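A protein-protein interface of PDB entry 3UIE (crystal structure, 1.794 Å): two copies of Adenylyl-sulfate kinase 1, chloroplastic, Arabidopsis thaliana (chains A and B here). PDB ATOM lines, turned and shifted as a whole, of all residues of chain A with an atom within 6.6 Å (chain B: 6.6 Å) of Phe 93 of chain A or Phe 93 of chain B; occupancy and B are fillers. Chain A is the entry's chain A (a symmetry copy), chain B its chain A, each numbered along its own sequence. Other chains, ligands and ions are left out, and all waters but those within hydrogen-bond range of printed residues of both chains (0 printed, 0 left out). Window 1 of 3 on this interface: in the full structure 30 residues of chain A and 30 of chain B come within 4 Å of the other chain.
Of the printed residues of chain B, Asp 95 of chain A touches Tyr 57. Printed residues of chain A within 4 Å of Val 89 of chain B: Val 89. Of the printed residues of chain A, Leu 92 of chain B touches Tyr 57 and Phe 93. Of chain A, only Leu 92 (3.8 Å), Phe 93 (3.8 Å) and Ala 96 (3.8 Å) come within 4 Å of Phe 93 of chain B. Printed residues of chain A within 4 Å of Asp 95 of chain B: Tyr 57.
The backbone NH (N) of Tyr 57 of chain B is in hydrogen-bond range of the backbone carbonyl oxygen (O) of Ile 99 of chain B (3.1 Å). N of Ile 98 of chain B lies within hydrogen-bond range of O of Phe 93 of chain B (3.0 Å). O of Ile 99 of chain A sits at hydrogen-bond distance from N of Tyr 57 of chain A, at 3.1 Å. The backbone carbonyl oxygen of Phe 93 of chain A lies within hydrogen-bond range of the backbone NH of Ile 98 of chain A, at 3.0 Å.
Hydrophobic or aromatic side chains of chain B that line the printed part of chain A: Tyr 57, Val 89, Leu 92, Phe 93 and Ala 96. Among the printed residues, 12 pairs touch across the chains. Among the printed residues, no Asp or Glu carboxylate lies within 4 Å of a Lys or Arg side-chain nitrogen of the other chain.
Among the printed residues, pairs that only touch across the chains: Tyr 57 of chain A with Leu 92 of chain B, Tyr 57 of chain A with Ala 96 of chain B, Val 89 of chain A with Val 89 of chain B, Leu 92 of chain A with Tyr 57 of chain B, Leu 92 of chain A with Phe 93 of chain B, Phe 93 of chain A with Leu 92 of chain B, Phe 93 of chain A with Phe 93 of chain B, Phe 93 of chain A with Ala 96 of chain B, Ala 96 of chain A with Tyr 57 of chain B and Ala 96 of chain A with Phe 93 of chain B.
OD2 of Asp 95 of chain A lies within hydrogen-bond range of OH of Tyr 57 of chain B, 2.7 Å away. OD2 of Asp 95 of chain B sits at hydrogen-bond distance from OH of Tyr 57 of chain A (2.7 Å).
Tyr 57 of chain A touches Asp 95 of chain B, and with the chains exchanged Asp 95 of chain A touches Tyr 57 of chain B. Leu 92 of chain A touches Phe 93 of chain B, and with the chains exchanged Phe 93 of chain A touches Leu 92 of chain B. Phe 93 of chain A touches its own counterpart, Phe 93 of chain B. Phe 93 of chain A touches Ala 96 of chain B, and with the chains exchanged Ala 96 of chain A touches Phe 93 of chain B.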
ATOM      1  N   GLY A  25     -25.342  10.658 -19.517  1.00  0.00           N
ATOM      2  CA  GLY A  25     -23.994  10.685 -18.990  1.00  0.00           C
ATOM      3  C   GLY A  25     -24.053  11.023 -17.512  1.00  0.00           C
ATOM      4  O   GLY A  25     -24.873  11.831 -17.090  1.00  0.00           O
ATOM      5  N   CYS A  26     -23.198  10.402 -16.715  1.00  0.00           N
ATOM      6  CA  CYS A  26     -23.197  10.690 -15.289  1.00  0.00           C
ATOM      7  C   CYS A  26     -21.922  10.154 -14.682  1.00  0.00           C
ATOM      8  O   CYS A  26     -21.162   9.459 -15.351  1.00  0.00           O
ATOM      9  CB  CYS A  26     -24.428  10.085 -14.599  1.00  0.00           C
ATOM     10  SG  CYS A  26     -24.650   8.297 -14.867  1.00  0.00           S
ATOM     11  N   VAL A  27     -21.681  10.496 -13.422  1.00  0.00           N
ATOM     12  CA  VAL A  27     -20.524   9.984 -12.702  1.00  0.00           C
ATOM     13  C   VAL A  27     -21.017   9.189 -11.502  1.00  0.00           C
ATOM     14  O   VAL A  27     -21.761   9.723 -10.686  1.00  0.00           O
ATOM     15  CB  VAL A  27     -19.658  11.137 -12.179  1.00  0.00           C
ATOM     16  CG1 VAL A  27     -18.493  10.583 -11.369  1.00  0.00           C
ATOM     17  CG2 VAL A  27     -19.167  12.014 -13.353  1.00  0.00           C
ATOM     18  N   TYR A  57     -17.829   3.207 -18.350  1.00  0.00           N
ATOM     19  CA  TYR A  57     -16.374   3.112 -18.361  1.00  0.00           C
ATOM     20  C   TYR A  57     -15.868   3.327 -16.939  1.00  0.00           C
ATOM     21  O   TYR A  57     -16.261   4.285 -16.291  1.00  0.00           O
ATOM     22  CB  TYR A  57     -15.753   4.135 -19.308  1.00  0.00           C
ATOM     23  CG  TYR A  57     -14.300   3.798 -19.528  1.00  0.00           C
ATOM     24  CD1 TYR A  57     -13.934   2.717 -20.329  1.00  0.00           C
ATOM     25  CD2 TYR A  57     -13.300   4.516 -18.889  1.00  0.00           C
ATOM     26  CE1 TYR A  57     -12.592   2.382 -20.505  1.00  0.00           C
ATOM     27  CE2 TYR A  57     -11.971   4.188 -19.048  1.00  0.00           C
ATOM     28  CZ  TYR A  57     -11.622   3.128 -19.861  1.00  0.00           C
ATOM     29  OH  TYR A  57     -10.295   2.812 -20.012  1.00  0.00           O
ATOM     30  N   LEU A  59     -13.094   4.278 -14.191  1.00  0.00           N
ATOM     31  CA  LEU A  59     -11.839   4.915 -13.827  1.00  0.00           C
ATOM     32  C   LEU A  59     -11.422   4.404 -12.456  1.00  0.00           C
ATOM     33  O   LEU A  59     -11.896   4.894 -11.434  1.00  0.00           O
ATOM     34  CB  LEU A  59     -12.003   6.439 -13.768  1.00  0.00           C
ATOM     35  CG  LEU A  59     -12.452   7.128 -15.053  1.00  0.00           C
ATOM     36  CD1 LEU A  59     -12.625   8.636 -14.832  1.00  0.00           C
ATOM     37  CD2 LEU A  59     -11.451   6.836 -16.176  1.00  0.00           C
ATOM     38  N   GLU A  88     -12.241  15.517 -12.863  1.00  0.00           N
ATOM     39  CA  GLU A  88     -12.281  16.234 -14.137  1.00  0.00           C
ATOM     40  C   GLU A  88     -12.439  15.276 -15.319  1.00  0.00           C
ATOM     41  O   GLU A  88     -13.177  15.551 -16.266  1.00  0.00           O
ATOM     42  CB  GLU A  88     -11.040  17.119 -14.305  1.00  0.00           C
ATOM     43  CG  GLU A  88     -11.006  18.334 -13.332  1.00  0.00           C
ATOM     44  CD  GLU A  88     -11.868  19.525 -13.778  1.00  0.00           C
ATOM     45  OE1 GLU A  88     -12.725  19.400 -14.690  1.00  0.00           O
ATOM     46  OE2 GLU A  88     -11.685  20.619 -13.204  1.00  0.00           O
ATOM     47  N   VAL A  89     -11.750  14.149 -15.266  1.00  0.00           N
ATOM     48  CA  VAL A  89     -11.882  13.178 -16.353  1.00  0.00           C
ATOM     49  C   VAL A  89     -13.270  12.541 -16.356  1.00  0.00           C
ATOM     50  O   VAL A  89     -13.881  12.357 -17.410  1.00  0.00           O
ATOM     51  CB  VAL A  89     -10.793  12.115 -16.280  1.00  0.00           C
ATOM     52  CG1 VAL A  89     -11.055  11.018 -17.323  1.00  0.00           C
ATOM     53  CG2 VAL A  89      -9.425  12.775 -16.525  1.00  0.00           C
ATOM     54  N   ALA A  90     -13.780  12.226 -15.166  1.00  0.00           N
ATOM     55  CA  ALA A  90     -15.133  11.691 -15.039  1.00  0.00           C
ATOM     56  C   ALA A  90     -16.159  12.656 -15.636  1.00  0.00           C
ATOM     57  O   ALA A  90     -17.127  12.248 -16.267  1.00  0.00           O
ATOM     58  CB  ALA A  90     -15.453  11.415 -13.577  1.00  0.00           C
ATOM     59  N   LYS A  91     -15.945  13.947 -15.423  1.00  0.00           N
ATOM     60  CA  LYS A  91     -16.829  14.954 -15.971  1.00  0.00           C
ATOM     61  C   LYS A  91     -16.810  14.920 -17.498  1.00  0.00           C
ATOM     62  O   LYS A  91     -17.846  15.066 -18.139  1.00  0.00           O
ATOM     63  CB  LYS A  91     -16.423  16.336 -15.464  1.00  0.00           C
ATOM     64  CG  LYS A  91     -17.160  17.466 -16.142  1.00  0.00           C
ATOM     65  CD  LYS A  91     -16.829  18.774 -15.479  1.00  0.00           C
ATOM     66  CE  LYS A  91     -17.574  19.923 -16.121  1.00  0.00           C
ATOM     67  NZ  LYS A  91     -17.285  21.199 -15.411  1.00  0.00           N
ATOM     68  N   LEU A  92     -15.625  14.735 -18.083  1.00  0.00           N
ATOM     69  CA  LEU A  92     -15.519  14.631 -19.540  1.00  0.00           C
ATOM     70  C   LEU A  92     -16.270  13.393 -20.055  1.00  0.00           C
ATOM     71  O   LEU A  92     -16.982  13.461 -21.066  1.00  0.00           O
ATOM     72  CB  LEU A  92     -14.051  14.581 -19.980  1.00  0.00           C
ATOM     73  CG  LEU A  92     -13.193  15.788 -19.597  1.00  0.00           C
ATOM     74  CD1 LEU A  92     -11.722  15.524 -19.913  1.00  0.00           C
ATOM     75  CD2 LEU A  92     -13.681  17.055 -20.302  1.00  0.00           C
ATOM     76  N   PHE A  93     -16.123  12.268 -19.362  1.00  0.00           N
ATOM     77  CA  PHE A  93     -16.858  11.072 -19.764  1.00  0.00           C
ATOM     78  C   PHE A  93     -18.370  11.245 -19.671  1.00  0.00           C
ATOM     79  O   PHE A  93     -19.117  10.787 -20.545  1.00  0.00           O
ATOM     80  CB  PHE A  93     -16.421   9.845 -18.958  1.00  0.00           C
ATOM     81  CG  PHE A  93     -15.227   9.140 -19.548  1.00  0.00           C
ATOM     82  CD1 PHE A  93     -15.393   8.148 -20.499  1.00  0.00           C
ATOM     83  CD2 PHE A  93     -13.946   9.484 -19.167  1.00  0.00           C
ATOM     84  CE1 PHE A  93     -14.298   7.497 -21.050  1.00  0.00           C
ATOM     85  CE2 PHE A  93     -12.840   8.828 -19.711  1.00  0.00           C
ATOM     86  CZ  PHE A  93     -13.023   7.833 -20.653  1.00  0.00           C
ATOM     87  N   ALA A  94     -18.824  11.864 -18.588  1.00  0.00           N
ATOM     88  CA  ALA A  94     -20.241  12.168 -18.437  1.00  0.00           C
ATOM     89  C   ALA A  94     -20.712  13.071 -19.573  1.00  0.00           C
ATOM     90  O   ALA A  94     -21.818  12.907 -20.097  1.00  0.00           O
ATOM     91  CB  ALA A  94     -20.491  12.845 -17.062  1.00  0.00           C
ATOM     92  N   ASP A  95     -19.876  14.034 -19.960  1.00  0.00           N
ATOM     93  CA  ASP A  95     -20.252  14.961 -21.018  1.00  0.00           C
ATOM     94  C   ASP A  95     -20.327  14.224 -22.367  1.00  0.00           C
ATOM     95  O   ASP A  95     -21.112  14.591 -23.245  1.00  0.00           O
ATOM     96  CB  ASP A  95     -19.281  16.152 -21.068  1.00  0.00           C
ATOM     97  CG  ASP A  95     -19.723  17.226 -22.042  1.00  0.00           C
ATOM     98  OD1 ASP A  95     -20.915  17.593 -22.015  1.00  0.00           O
ATOM     99  OD2 ASP A  95     -18.874  17.702 -22.826  1.00  0.00           O
ATOM    100  N   ALA A  96     -19.558  13.148 -22.493  1.00  0.00           N
ATOM    101  CA  ALA A  96     -19.580  12.307 -23.692  1.00  0.00           C
ATOM    102  C   ALA A  96     -20.792  11.386 -23.716  1.00  0.00           C
ATOM    103  O   ALA A  96     -20.986  10.650 -24.688  1.00  0.00           O
ATOM    104  CB  ALA A  96     -18.314  11.486 -23.769  1.00  0.00           C
ATOM    105  N   GLY A  97     -21.571  11.390 -22.632  1.00  0.00           N
ATOM    106  CA  GLY A  97     -22.786  10.595 -22.527  1.00  0.00           C
ATOM    107  C   GLY A  97     -22.593   9.247 -21.841  1.00  0.00           C
ATOM    108  O   GLY A  97     -23.505   8.424 -21.801  1.00  0.00           O
ATOM    109  N   ILE A  98     -21.391   9.019 -21.319  1.00  0.00           N
ATOM    110  CA  ILE A  98     -21.003   7.743 -20.727  1.00  0.00           C
ATOM    111  C   ILE A  98     -21.389   7.696 -19.248  1.00  0.00           C
ATOM    112  O   ILE A  98     -21.343   8.714 -18.573  1.00  0.00           O
ATOM    113  CB  ILE A  98     -19.465   7.583 -20.811  1.00  0.00           C
ATOM    114  CG1 ILE A  98     -18.990   7.703 -22.261  1.00  0.00           C
ATOM    115  CG2 ILE A  98     -19.021   6.283 -20.178  1.00  0.00           C
ATOM    116  CD1 ILE A  98     -19.523   6.641 -23.145  1.00  0.00           C
ATOM    117  N   ILE A  99     -21.768   6.514 -18.761  1.00  0.00           N
ATOM    118  CA  ILE A  99     -21.928   6.281 -17.329  1.00  0.00           C
ATOM    119  C   ILE A  99     -20.543   5.975 -16.797  1.00  0.00           C
ATOM    120  O   ILE A  99     -20.012   4.879 -16.986  1.00  0.00           O
ATOM    121  CB  ILE A  99     -22.896   5.117 -17.054  1.00  0.00           C
ATOM    122  CG1 ILE A  99     -24.288   5.479 -17.591  1.00  0.00           C
ATOM    123  CG2 ILE A  99     -22.968   4.795 -15.533  1.00  0.00           C
ATOM    124  CD1 ILE A  99     -25.218   4.294 -17.811  1.00  0.00           C
ATOM    125  N   CYS A 100     -19.937   6.972 -16.166  1.00  0.00           N
ATOM    126  CA  CYS A 100     -18.551   6.849 -15.728  1.00  0.00           C
ATOM    127  C   CYS A 100     -18.489   6.406 -14.276  1.00  0.00           C
ATOM    128  O   CYS A 100     -19.007   7.094 -13.398  1.00  0.00           O
ATOM    129  CB  CYS A 100     -17.834   8.201 -15.892  1.00  0.00           C
ATOM    130  SG  CYS A 100     -16.072   8.117 -15.521  1.00  0.00           S
ATOM    131  N   GLY B  25     -12.579   2.331 -31.098  1.00  0.00           N
ATOM    132  CA  GLY B  25     -12.019   3.418 -30.324  1.00  0.00           C
ATOM    133  C   GLY B  25     -10.691   3.821 -30.937  1.00  0.00           C
ATOM    134  O   GLY B  25      -9.938   2.974 -31.404  1.00  0.00           O
ATOM    135  N   CYS B  26     -10.399   5.112 -30.951  1.00  0.00           N
ATOM    136  CA  CYS B  26      -9.135   5.562 -31.514  1.00  0.00           C
ATOM    137  C   CYS B  26      -8.886   6.988 -31.081  1.00  0.00           C
ATOM    138  O   CYS B  26      -9.759   7.617 -30.490  1.00  0.00           O
ATOM    139  CB  CYS B  26      -9.137   5.447 -33.045  1.00  0.00           C
ATOM    140  SG  CYS B  26     -10.519   6.298 -33.872  1.00  0.00           S
ATOM    141  N   VAL B  27      -7.688   7.486 -31.359  1.00  0.00           N
ATOM    142  CA  VAL B  27      -7.351   8.870 -31.061  1.00  0.00           C
ATOM    143  C   VAL B  27      -7.011   9.575 -32.365  1.00  0.00           C
ATOM    144  O   VAL B  27      -6.129   9.122 -33.087  1.00  0.00           O
ATOM    145  CB  VAL B  27      -6.117   8.943 -30.152  1.00  0.00           C
ATOM    146  CG1 VAL B  27      -5.739  10.399 -29.909  1.00  0.00           C
ATOM    147  CG2 VAL B  27      -6.385   8.197 -28.825  1.00  0.00           C
ATOM    148  N   TYR B  57     -15.709  12.340 -29.276  1.00  0.00           N
ATOM    149  CA  TYR B  57     -15.623  13.336 -28.213  1.00  0.00           C
ATOM    150  C   TYR B  57     -14.355  14.156 -28.426  1.00  0.00           C
ATOM    151  O   TYR B  57     -13.288  13.592 -28.614  1.00  0.00           O
ATOM    152  CB  TYR B  57     -15.610  12.683 -26.834  1.00  0.00           C
ATOM    153  CG  TYR B  57     -15.839  13.735 -25.778  1.00  0.00           C
ATOM    154  CD1 TYR B  57     -17.103  14.291 -25.590  1.00  0.00           C
ATOM    155  CD2 TYR B  57     -14.784  14.216 -25.017  1.00  0.00           C
ATOM    156  CE1 TYR B  57     -17.308  15.290 -24.640  1.00  0.00           C
ATOM    157  CE2 TYR B  57     -14.974  15.209 -24.080  1.00  0.00           C
ATOM    158  CZ  TYR B  57     -16.235  15.736 -23.889  1.00  0.00           C
ATOM    159  OH  TYR B  57     -16.412  16.725 -22.954  1.00  0.00           O
ATOM    160  N   LEU B  59     -11.367  16.569 -27.243  1.00  0.00           N
ATOM    161  CA  LEU B  59     -10.546  17.145 -26.191  1.00  0.00           C
ATOM    162  C   LEU B  59      -9.796  18.337 -26.766  1.00  0.00           C
ATOM    163  O   LEU B  59      -8.758  18.176 -27.403  1.00  0.00           O
ATOM    164  CB  LEU B  59      -9.534  16.116 -25.671  1.00  0.00           C
ATOM    165  CG  LEU B  59     -10.107  14.830 -25.084  1.00  0.00           C
ATOM    166  CD1 LEU B  59      -8.983  13.877 -24.656  1.00  0.00           C
ATOM    167  CD2 LEU B  59     -11.036  15.163 -23.912  1.00  0.00           C
ATOM    168  N   GLU B  88      -3.007  10.710 -22.286  1.00  0.00           N
ATOM    169  CA  GLU B  88      -3.510   9.676 -21.383  1.00  0.00           C
ATOM    170  C   GLU B  88      -5.039   9.649 -21.351  1.00  0.00           C
ATOM    171  O   GLU B  88      -5.655   8.583 -21.328  1.00  0.00           O
ATOM    172  CB  GLU B  88      -2.931   9.854 -19.974  1.00  0.00           C
ATOM    173  CG  GLU B  88      -1.407   9.548 -19.884  1.00  0.00           C
ATOM    174  CD  GLU B  88      -1.066   8.053 -19.793  1.00  0.00           C
ATOM    175  OE1 GLU B  88      -1.928   7.175 -20.053  1.00  0.00           O
ATOM    176  OE2 GLU B  88       0.094   7.744 -19.450  1.00  0.00           O
ATOM    177  N   VAL B  89      -5.653  10.820 -21.353  1.00  0.00           N
ATOM    178  CA  VAL B  89      -7.116  10.859 -21.354  1.00  0.00           C
ATOM    179  C   VAL B  89      -7.679  10.357 -22.682  1.00  0.00           C
ATOM    180  O   VAL B  89      -8.660   9.612 -22.714  1.00  0.00           O
ATOM    181  CB  VAL B  89      -7.632  12.257 -21.037  1.00  0.00           C
ATOM    182  CG1 VAL B  89      -9.157  12.311 -21.213  1.00  0.00           C
ATOM    183  CG2 VAL B  89      -7.243  12.623 -19.593  1.00  0.00           C
ATOM    184  N   ALA B  90      -7.039  10.748 -23.784  1.00  0.00           N
ATOM    185  CA  ALA B  90      -7.434  10.262 -25.103  1.00  0.00           C
ATOM    186  C   ALA B  90      -7.371   8.735 -25.162  1.00  0.00           C
ATOM    187  O   ALA B  90      -8.215   8.085 -25.768  1.00  0.00           O
ATOM    188  CB  ALA B  90      -6.543  10.872 -26.175  1.00  0.00           C
ATOM    189  N   LYS B  91      -6.352   8.164 -24.535  1.00  0.00           N
ATOM    190  CA  LYS B  91      -6.211   6.724 -24.493  1.00  0.00           C
ATOM    191  C   LYS B  91      -7.384   6.084 -23.753  1.00  0.00           C
ATOM    192  O   LYS B  91      -7.885   5.041 -24.160  1.00  0.00           O
ATOM    193  CB  LYS B  91      -4.890   6.350 -23.822  1.00  0.00           C
ATOM    194  CG  LYS B  91      -4.750   4.871 -23.552  1.00  0.00           C
ATOM    195  CD  LYS B  91      -3.369   4.563 -23.046  1.00  0.00           C
ATOM    196  CE  LYS B  91      -3.191   3.083 -22.792  1.00  0.00           C
ATOM    197  NZ  LYS B  91      -1.799   2.788 -22.355  1.00  0.00           N
ATOM    198  N   LEU B  92      -7.818   6.707 -22.657  1.00  0.00           N
ATOM    199  CA  LEU B  92      -8.974   6.197 -21.916  1.00  0.00           C
ATOM    200  C   LEU B  92     -10.244   6.256 -22.779  1.00  0.00           C
ATOM    201  O   LEU B  92     -11.040   5.307 -22.797  1.00  0.00           O
ATOM    202  CB  LEU B  92      -9.181   6.984 -20.616  1.00  0.00           C
ATOM    203  CG  LEU B  92      -8.019   6.956 -19.621  1.00  0.00           C
ATOM    204  CD1 LEU B  92      -8.271   7.932 -18.473  1.00  0.00           C
ATOM    205  CD2 LEU B  92      -7.785   5.540 -19.089  1.00  0.00           C
ATOM    206  N   PHE B  93     -10.432   7.357 -23.500  1.00  0.00           N
ATOM    207  CA  PHE B  93     -11.588   7.449 -24.388  1.00  0.00           C
ATOM    208  C   PHE B  93     -11.569   6.405 -25.499  1.00  0.00           C
ATOM    209  O   PHE B  93     -12.604   5.821 -25.841  1.00  0.00           O
ATOM    210  CB  PHE B  93     -11.726   8.850 -24.990  1.00  0.00           C
ATOM    211  CG  PHE B  93     -12.499   9.801 -24.113  1.00  0.00           C
ATOM    212  CD1 PHE B  93     -13.876   9.892 -24.215  1.00  0.00           C
ATOM    213  CD2 PHE B  93     -11.852  10.584 -23.178  1.00  0.00           C
ATOM    214  CE1 PHE B  93     -14.596  10.762 -23.408  1.00  0.00           C
ATOM    215  CE2 PHE B  93     -12.568  11.467 -22.368  1.00  0.00           C
ATOM    216  CZ  PHE B  93     -13.942  11.552 -22.490  1.00  0.00           C
ATOM    217  N   ALA B  94     -10.399   6.204 -26.094  1.00  0.00           N
ATOM    218  CA  ALA B  94     -10.240   5.165 -27.103  1.00  0.00           C
ATOM    219  C   ALA B  94     -10.565   3.797 -26.510  1.00  0.00           C
ATOM    220  O   ALA B  94     -11.185   2.953 -27.163  1.00  0.00           O
ATOM    221  CB  ALA B  94      -8.791   5.188 -27.661  1.00  0.00           C
ATOM    222  N   ASP B  95     -10.145   3.567 -25.266  1.00  0.00           N
ATOM    223  CA  ASP B  95     -10.385   2.281 -24.629  1.00  0.00           C
ATOM    224  C   ASP B  95     -11.889   2.096 -24.357  1.00  0.00           C
ATOM    225  O   ASP B  95     -12.399   0.973 -24.362  1.00  0.00           O
ATOM    226  CB  ASP B  95      -9.549   2.145 -23.346  1.00  0.00           C
ATOM    227  CG  ASP B  95      -9.637   0.761 -22.733  1.00  0.00           C
ATOM    228  OD1 ASP B  95      -9.508  -0.226 -23.485  1.00  0.00           O
ATOM    229  OD2 ASP B  95      -9.830   0.668 -21.502  1.00  0.00           O
ATOM    230  N   ALA B  96     -12.597   3.207 -24.189  1.00  0.00           N
ATOM    231  CA  ALA B  96     -14.049   3.188 -23.996  1.00  0.00           C
ATOM    232  C   ALA B  96     -14.792   2.967 -25.306  1.00  0.00           C
ATOM    233  O   ALA B  96     -16.023   2.871 -25.306  1.00  0.00           O
ATOM    234  CB  ALA B  96     -14.502   4.483 -23.364  1.00  0.00           C
ATOM    235  N   GLY B  97     -14.054   2.939 -26.417  1.00  0.00           N
ATOM    236  CA  GLY B  97     -14.619   2.695 -27.737  1.00  0.00           C
ATOM    237  C   GLY B  97     -14.952   3.961 -28.518  1.00  0.00           C
ATOM    238  O   GLY B  97     -15.552   3.902 -29.589  1.00  0.00           O
ATOM    239  N   ILE B  98     -14.576   5.110 -27.964  1.00  0.00           N
ATOM    240  CA  ILE B  98     -14.912   6.417 -28.520  1.00  0.00           C
ATOM    241  C   ILE B  98     -13.867   6.848 -29.549  1.00  0.00           C
ATOM    242  O   ILE B  98     -12.695   6.542 -29.393  1.00  0.00           O
ATOM    243  CB  ILE B  98     -14.914   7.473 -27.389  1.00  0.00           C
ATOM    244  CG1 ILE B  98     -15.881   7.067 -26.274  1.00  0.00           C
ATOM    245  CG2 ILE B  98     -15.229   8.849 -27.933  1.00  0.00           C
ATOM    246  CD1 ILE B  98     -17.293   6.993 -26.716  1.00  0.00           C
ATOM    247  N   ILE B  99     -14.304   7.554 -30.593  1.00  0.00           N
ATOM    248  CA  ILE B  99     -13.390   8.227 -31.511  1.00  0.00           C
ATOM    249  C   ILE B  99     -13.038   9.548 -30.857  1.00  0.00           C
ATOM    250  O   ILE B  99     -13.832  10.490 -30.848  1.00  0.00           O
ATOM    251  CB  ILE B  99     -14.039   8.447 -32.888  1.00  0.00           C
ATOM    252  CG1 ILE B  99     -14.359   7.085 -33.520  1.00  0.00           C
ATOM    253  CG2 ILE B  99     -13.106   9.272 -33.823  1.00  0.00           C
ATOM    254  CD1 ILE B  99     -15.392   7.125 -34.639  1.00  0.00           C
ATOM    255  N   CYS B 100     -11.851   9.597 -30.266  1.00  0.00           N
ATOM    256  CA  CYS B 100     -11.451  10.762 -29.486  1.00  0.00           C
ATOM    257  C   CYS B 100     -10.635  11.720 -30.338  1.00  0.00           C
ATOM    258  O   CYS B 100      -9.582  11.344 -30.852  1.00  0.00           O
ATOM    259  CB  CYS B 100     -10.624  10.313 -28.269  1.00  0.00           C
ATOM    260  SG  CYS B 100     -10.209  11.668 -27.155  1.00  0.00           S
